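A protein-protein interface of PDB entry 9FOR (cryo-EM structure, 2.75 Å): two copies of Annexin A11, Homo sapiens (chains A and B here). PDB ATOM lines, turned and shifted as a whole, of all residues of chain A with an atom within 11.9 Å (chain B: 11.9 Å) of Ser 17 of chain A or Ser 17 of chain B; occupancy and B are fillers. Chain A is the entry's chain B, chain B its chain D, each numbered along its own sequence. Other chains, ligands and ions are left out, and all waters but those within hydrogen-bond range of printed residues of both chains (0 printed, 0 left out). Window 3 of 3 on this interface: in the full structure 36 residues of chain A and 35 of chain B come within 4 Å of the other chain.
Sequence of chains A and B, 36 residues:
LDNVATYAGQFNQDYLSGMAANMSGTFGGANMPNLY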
ATOM      1  N   ASN A  12      -2.877 -20.277 -16.534  1.00  0.00           N
ATOM      2  CA  ASN A  12      -3.196 -19.221 -15.582  1.00  0.00           C
ATOM      3  C   ASN A  12      -2.254 -19.267 -14.377  1.00  0.00           C
ATOM      4  O   ASN A  12      -2.363 -20.163 -13.547  1.00  0.00           O
ATOM      5  CB  ASN A  12      -4.647 -19.317 -15.123  1.00  0.00           C
ATOM      6  CG  ASN A  12      -5.603 -19.281 -16.297  1.00  0.00           C
ATOM      7  OD1 ASN A  12      -5.616 -18.309 -17.055  1.00  0.00           O
ATOM      8  ND2 ASN A  12      -6.398 -20.323 -16.489  1.00  0.00           N
ATOM      9  N   GLN A  13      -1.350 -18.281 -14.262  1.00  0.00           N
ATOM     10  CA  GLN A  13      -0.221 -18.365 -13.357  1.00  0.00           C
ATOM     11  C   GLN A  13       0.173 -16.982 -12.827  1.00  0.00           C
ATOM     12  O   GLN A  13       1.329 -16.588 -12.943  1.00  0.00           O
ATOM     13  CB  GLN A  13       0.950 -19.060 -14.057  1.00  0.00           C
ATOM     14  CG  GLN A  13       0.761 -20.556 -14.330  1.00  0.00           C
ATOM     15  CD  GLN A  13       1.860 -21.190 -15.159  1.00  0.00           C
ATOM     16  OE1 GLN A  13       2.594 -20.517 -15.882  1.00  0.00           O
ATOM     17  NE2 GLN A  13       1.965 -22.508 -15.128  1.00  0.00           N
ATOM     18  N   ASP A  14      -0.737 -16.278 -12.143  1.00  0.00           N
ATOM     19  CA  ASP A  14      -0.384 -15.032 -11.476  1.00  0.00           C
ATOM     20  C   ASP A  14       0.355 -15.233 -10.146  1.00  0.00           C
ATOM     21  O   ASP A  14       0.248 -16.264  -9.485  1.00  0.00           O
ATOM     22  CB  ASP A  14      -1.581 -14.122 -11.275  1.00  0.00           C
ATOM     23  CG  ASP A  14      -2.178 -13.554 -12.558  1.00  0.00           C
ATOM     24  OD1 ASP A  14      -1.679 -13.914 -13.656  1.00  0.00           O
ATOM     25  OD2 ASP A  14      -3.138 -12.755 -12.456  1.00  0.00           O
ATOM     26  N   TYR A  15       1.150 -14.205  -9.801  1.00  0.00           N
ATOM     27  CA  TYR A  15       2.043 -14.162  -8.651  1.00  0.00           C
ATOM     28  C   TYR A  15       2.974 -15.376  -8.523  1.00  0.00           C
ATOM     29  O   TYR A  15       3.117 -15.913  -7.437  1.00  0.00           O
ATOM     30  CB  TYR A  15       1.226 -13.998  -7.379  1.00  0.00           C
ATOM     31  CG  TYR A  15       0.323 -12.786  -7.412  1.00  0.00           C
ATOM     32  CD1 TYR A  15       0.794 -11.538  -7.034  1.00  0.00           C
ATOM     33  CD2 TYR A  15      -0.998 -12.893  -7.816  1.00  0.00           C
ATOM     34  CE1 TYR A  15      -0.023 -10.417  -7.066  1.00  0.00           C
ATOM     35  CE2 TYR A  15      -1.830 -11.783  -7.845  1.00  0.00           C
ATOM     36  CZ  TYR A  15      -1.340 -10.542  -7.470  1.00  0.00           C
ATOM     37  OH  TYR A  15      -2.153  -9.448  -7.495  1.00  0.00           O
ATOM     38  N   LEU A  16       3.706 -15.741  -9.569  1.00  0.00           N
ATOM     39  CA  LEU A  16       4.614 -16.878  -9.509  1.00  0.00           C
ATOM     40  C   LEU A  16       5.929 -16.492  -8.849  1.00  0.00           C
ATOM     41  O   LEU A  16       6.627 -15.598  -9.319  1.00  0.00           O
ATOM     42  CB  LEU A  16       4.857 -17.356 -10.933  1.00  0.00           C
ATOM     43  CG  LEU A  16       5.584 -18.676 -11.108  1.00  0.00           C
ATOM     44  CD1 LEU A  16       5.274 -19.228 -12.485  1.00  0.00           C
ATOM     45  CD2 LEU A  16       7.053 -18.460 -10.970  1.00  0.00           C
ATOM     46  N   SER A  17       6.330 -17.232  -7.810  1.00  0.00           N
ATOM     47  CA  SER A  17       7.627 -16.987  -7.204  1.00  0.00           C
ATOM     48  C   SER A  17       8.521 -18.231  -7.129  1.00  0.00           C
ATOM     49  O   SER A  17       9.655 -18.107  -6.691  1.00  0.00           O
ATOM     50  CB  SER A  17       7.441 -16.376  -5.877  1.00  0.00           C
ATOM     51  OG  SER A  17       6.885 -17.312  -4.983  1.00  0.00           O
ATOM     52  N   GLY A  18       8.064 -19.394  -7.616  1.00  0.00           N
ATOM     53  CA  GLY A  18       8.908 -20.576  -7.740  1.00  0.00           C
ATOM     54  C   GLY A  18       9.392 -20.806  -9.169  1.00  0.00           C
ATOM     55  O   GLY A  18       9.930 -19.890  -9.762  1.00  0.00           O
ATOM     56  N   MET A  19       9.221 -22.019  -9.707  1.00  0.00           N
ATOM     57  CA  MET A  19       9.709 -22.403 -11.031  1.00  0.00           C
ATOM     58  C   MET A  19       8.636 -23.179 -11.812  1.00  0.00           C
ATOM     59  O   MET A  19       8.087 -24.138 -11.288  1.00  0.00           O
ATOM     60  CB  MET A  19      10.917 -23.347 -10.921  1.00  0.00           C
ATOM     61  CG  MET A  19      12.048 -22.838 -10.029  1.00  0.00           C
ATOM     62  SD  MET A  19      13.480 -23.931  -9.776  1.00  0.00           S
ATOM     63  CE  MET A  19      14.438 -24.086 -11.282  1.00  0.00           C
ATOM     64  N   ALA A  20       8.368 -22.820 -13.075  1.00  0.00           N
ATOM     65  CA  ALA A  20       7.395 -23.519 -13.920  1.00  0.00           C
ATOM     66  C   ALA A  20       7.972 -23.818 -15.301  1.00  0.00           C
ATOM     67  O   ALA A  20       8.653 -22.980 -15.871  1.00  0.00           O
ATOM     68  CB  ALA A  20       6.152 -22.682 -14.092  1.00  0.00           C
ATOM     69  N   ALA A  21       7.641 -24.980 -15.852  1.00  0.00           N
ATOM     70  CA  ALA A  21       8.014 -25.340 -17.209  1.00  0.00           C
ATOM     71  C   ALA A  21       6.769 -25.723 -18.026  1.00  0.00           C
ATOM     72  O   ALA A  21       6.138 -26.736 -17.743  1.00  0.00           O
ATOM     73  CB  ALA A  21       9.002 -26.482 -17.134  1.00  0.00           C
ATOM     74  N   ASN B  12      -0.987 -16.364 -19.155  1.00  0.00           N
ATOM     75  CA  ASN B  12      -1.343 -15.299 -18.227  1.00  0.00           C
ATOM     76  C   ASN B  12      -0.433 -15.317 -16.997  1.00  0.00           C
ATOM     77  O   ASN B  12      -0.553 -16.202 -16.157  1.00  0.00           O
ATOM     78  CB  ASN B  12      -2.804 -15.404 -17.803  1.00  0.00           C
ATOM     79  CG  ASN B  12      -3.729 -15.395 -19.003  1.00  0.00           C
ATOM     80  OD1 ASN B  12      -3.733 -14.435 -19.775  1.00  0.00           O
ATOM     81  ND2 ASN B  12      -4.507 -16.449 -19.201  1.00  0.00           N
ATOM     82  N   GLN B  13       0.456 -14.318 -16.873  1.00  0.00           N
ATOM     83  CA  GLN B  13       1.563 -14.378 -15.936  1.00  0.00           C
ATOM     84  C   GLN B  13       1.926 -12.983 -15.417  1.00  0.00           C
ATOM     85  O   GLN B  13       3.082 -12.577 -15.507  1.00  0.00           O
ATOM     86  CB  GLN B  13       2.760 -15.070 -16.596  1.00  0.00           C
ATOM     87  CG  GLN B  13       2.594 -16.571 -16.852  1.00  0.00           C
ATOM     88  CD  GLN B  13       3.721 -17.205 -17.643  1.00  0.00           C
ATOM     89  OE1 GLN B  13       4.467 -16.533 -18.356  1.00  0.00           O
ATOM     90  NE2 GLN B  13       3.840 -18.520 -17.589  1.00  0.00           N
ATOM     91  N   ASP B  14       0.992 -12.279 -14.767  1.00  0.00           N
ATOM     92  CA  ASP B  14       1.314 -11.020 -14.108  1.00  0.00           C
ATOM     93  C   ASP B  14       2.020 -11.193 -12.758  1.00  0.00           C
ATOM     94  O   ASP B  14       1.907 -12.217 -12.084  1.00  0.00           O
ATOM     95  CB  ASP B  14       0.103 -10.121 -13.952  1.00  0.00           C
ATOM     96  CG  ASP B  14      -0.467  -9.578 -15.259  1.00  0.00           C
ATOM     97  OD1 ASP B  14       0.065  -9.948 -16.338  1.00  0.00           O
ATOM     98  OD2 ASP B  14      -1.438  -8.788 -15.193  1.00  0.00           O
ATOM     99  N   TYR B  15       2.794 -10.152 -12.407  1.00  0.00           N
ATOM    100  CA  TYR B  15       3.656 -10.082 -11.235  1.00  0.00           C
ATOM    101  C   TYR B  15       4.597 -11.284 -11.064  1.00  0.00           C
ATOM    102  O   TYR B  15       4.716 -11.803  -9.968  1.00  0.00           O
ATOM    103  CB  TYR B  15       2.804  -9.910  -9.987  1.00  0.00           C
ATOM    104  CG  TYR B  15       1.890  -8.708 -10.061  1.00  0.00           C
ATOM    105  CD1 TYR B  15       2.336  -7.450  -9.689  1.00  0.00           C
ATOM    106  CD2 TYR B  15       0.580  -8.836 -10.498  1.00  0.00           C
ATOM    107  CE1 TYR B  15       1.508  -6.339  -9.758  1.00  0.00           C
ATOM    108  CE2 TYR B  15      -0.262  -7.736 -10.564  1.00  0.00           C
ATOM    109  CZ  TYR B  15       0.204  -6.484 -10.195  1.00  0.00           C
ATOM    110  OH  TYR B  15      -0.620  -5.400 -10.257  1.00  0.00           O
ATOM    111  N   LEU B  16       5.361 -11.656 -12.085  1.00  0.00           N
ATOM    112  CA  LEU B  16       6.278 -12.781 -11.985  1.00  0.00           C
ATOM    113  C   LEU B  16       7.571 -12.371 -11.297  1.00  0.00           C
ATOM    114  O   LEU B  16       8.271 -11.476 -11.761  1.00  0.00           O
ATOM    115  CB  LEU B  16       6.564 -13.276 -13.396  1.00  0.00           C
ATOM    116  CG  LEU B  16       7.309 -14.591 -13.532  1.00  0.00           C
ATOM    117  CD1 LEU B  16       7.042 -15.166 -14.909  1.00  0.00           C
ATOM    118  CD2 LEU B  16       8.772 -14.356 -13.359  1.00  0.00           C
ATOM    119  N   SER B  17       7.953 -13.092 -10.237  1.00  0.00           N
ATOM    120  CA  SER B  17       9.231 -12.824  -9.601  1.00  0.00           C
ATOM    121  C   SER B  17      10.136 -14.057  -9.485  1.00  0.00           C
ATOM    122  O   SER B  17      11.256 -13.912  -9.018  1.00  0.00           O
ATOM    123  CB  SER B  17       9.003 -12.196  -8.289  1.00  0.00           C
ATOM    124  OG  SER B  17       8.434 -13.125  -7.395  1.00  0.00           O
ATOM    125  N   GLY B  18       9.704 -15.231  -9.966  1.00  0.00           N
ATOM    126  CA  GLY B  18      10.564 -16.405 -10.051  1.00  0.00           C
ATOM    127  C   GLY B  18      11.088 -16.650 -11.464  1.00  0.00           C
ATOM    128  O   GLY B  18      11.631 -15.737 -12.055  1.00  0.00           O
ATOM    129  N   MET B  19      10.945 -17.872 -11.989  1.00  0.00           N
ATOM    130  CA  MET B  19      11.472 -18.270 -13.293  1.00  0.00           C
ATOM    131  C   MET B  19      10.427 -19.068 -14.091  1.00  0.00           C
ATOM    132  O   MET B  19       9.876 -20.026 -13.567  1.00  0.00           O
ATOM    133  CB  MET B  19      12.686 -19.198 -13.137  1.00  0.00           C
ATOM    134  CG  MET B  19      13.788 -18.664 -12.224  1.00  0.00           C
ATOM    135  SD  MET B  19      15.225 -19.737 -11.918  1.00  0.00           S
ATOM    136  CE  MET B  19      16.224 -19.903 -13.396  1.00  0.00           C
ATOM    137  N   ALA B  20      10.189 -18.730 -15.365  1.00  0.00           N
ATOM    138  CA  ALA B  20       9.247 -19.452 -16.225  1.00  0.00           C
ATOM    139  C   ALA B  20       9.863 -19.764 -17.585  1.00  0.00           C
ATOM    140  O   ALA B  20      10.549 -18.927 -18.150  1.00  0.00           O
ATOM    141  CB  ALA B  20       7.999 -18.632 -16.441  1.00  0.00           C
ATOM    142  N   ALA B  21       9.560 -20.938 -18.128  1.00  0.00           N
ATOM    143  CA  ALA B  21       9.972 -21.313 -19.470  1.00  0.00           C
ATOM    144  C   ALA B  21       8.754 -21.722 -20.314  1.00  0.00           C
ATOM    145  O   ALA B  21       8.126 -22.737 -20.032  1.00  0.00           O
ATOM    146  CB  ALA B  21      10.970 -22.442 -19.353  1.00  0.00           C
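OE1 of Gln 13 of chain A lies within hydrogen-bond range of NE2 of Gln 13 of chain B (2.9 Å). The backbone NH (N) of Ala 21 of chain B is in hydrogen-bond range of the backbone carbonyl oxygen (O) of Ala 20 of chain A (3.2 Å). The backbone NH of Tyr 15 of chain A sits at hydrogen-bond distance from the backbone carbonyl oxygen of Asp 14 of chain B, at 3.1 Å. The backbone carbonyl oxygen (O) of Leu 16 of chain A sits at hydrogen-bond distance from the backbone NH (N) of Gly 18 of chain B. The backbone carbonyl oxygen (O) of Leu 16 of chain A sits at hydrogen-bond distance from the backbone NH (N) of Ser 17 of chain B, 3.0 Å away. OD1 of Asn 12 of chain A lies within hydrogen-bond range of ND2 of Asn 12 of chain B, 3.0 Å away. The backbone NH of Met 19 of chain B sits at hydrogen-bond distance from the backbone carbonyl oxygen of Gly 18 of chain A (3.2 Å). N of Ala 20 of chain A is in hydrogen-bond range of O of Met 19 of chain B, at 3.2 Å. The side-chain carboxylate (OD1) of Asp 14 of chain A lies within hydrogen-bond range of the backbone NH (N) of Asp 14 of chain B, 3.3 Å away. The backbone carbonyl oxygen (O) of Asn 12 of chain B is in hydrogen-bond range of the backbone NH (N) of Gln 13 of chain A, 2.9 Å away.
Asn 12 of chain B touches Asp 14 of chain A. Asp 14 of chain A touches Gln 13 of chain B (OD1 to N, 3.9 Å). Tyr 15 of chain B touches Tyr 15 of chain A. Leu 16 of chain B touches Leu 16 of chain A. Ser 17 of chain B touches Ser 17 of chain A. Ser 17 of chain A touches Gly 18 of chain B. Gly 18 of chain B touches Gly 18 of chain A. Met 19 of chain A touches Met 19 of chain B (CA to O, 3.5 Å). Ala 20 of chain B touches Ala 20 of chain A. CA of Ala 21 of chain A touches O of Ala 21 of chain B, 3.8 Å away.
Of chain B, only Leu 16 (3.9 Å), Ser 17 (3.0 Å) and Gly 18 (3.2 Å) come within 4 Å of Leu 16 of chain A. Of the printed residues of chain B, Ser 17 of chain A touches Ser 17 (3.7 Å) and Gly 18 (3.9 Å). Printed residues of chain A within 4 Å of Gln 13 of chain B: Gln 13 (2.9 Å) and Asp 14 (3.9 Å). Leu 16 of chain B touches just one residue of chain A: Leu 16 (3.9 Å). Of chain A, only Leu 16 and Ser 17 come within 4 Å of Ser 17 of chain B. Gly 18 of chain B touches just these residues of chain A: Leu 16 (3.2 Å), Ser 17 (3.9 Å) and Gly 18 (3.6 Å). Printed residues of chain A within 4 Å of Ala 20 of chain B: Ala 20 (3.6 Å). The nearest residue of chain B that does not touch Ser 17 of chain A is Met 19 of chain B (5.4 Å).
Of the 10 printed residues of chain B, 10 touch a printed residue of chain A. Along chain B the printed residues that touch a printed residue of chain A span positions 12 to 21. Along chain A the printed residues that touch a printed residue of chain B span positions 12 to 21. Among the printed residues, 20 pairs touch across the chains.
Tyr 15 of chain B touches its own counterpart, Tyr 15 of chain A. Ser 17 of chain B touches its own counterpart, Ser 17 of chain A. Ser 17 of chain A touches Gly 18 of chain B, but with the chains exchanged Gly 18 of chain A does not touch Ser 17 of chain B (5.8 Å). Gly 18 of chain B touches its own counterpart, Gly 18 of chain A. Positions printed for both chains: 12, 13, 14, 15, 16, 17, 18, 19, 20 and 21. Of the 20 pairs that touch across the chains among the printed residues, 10 have their exchanged pair printed and touching as well.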
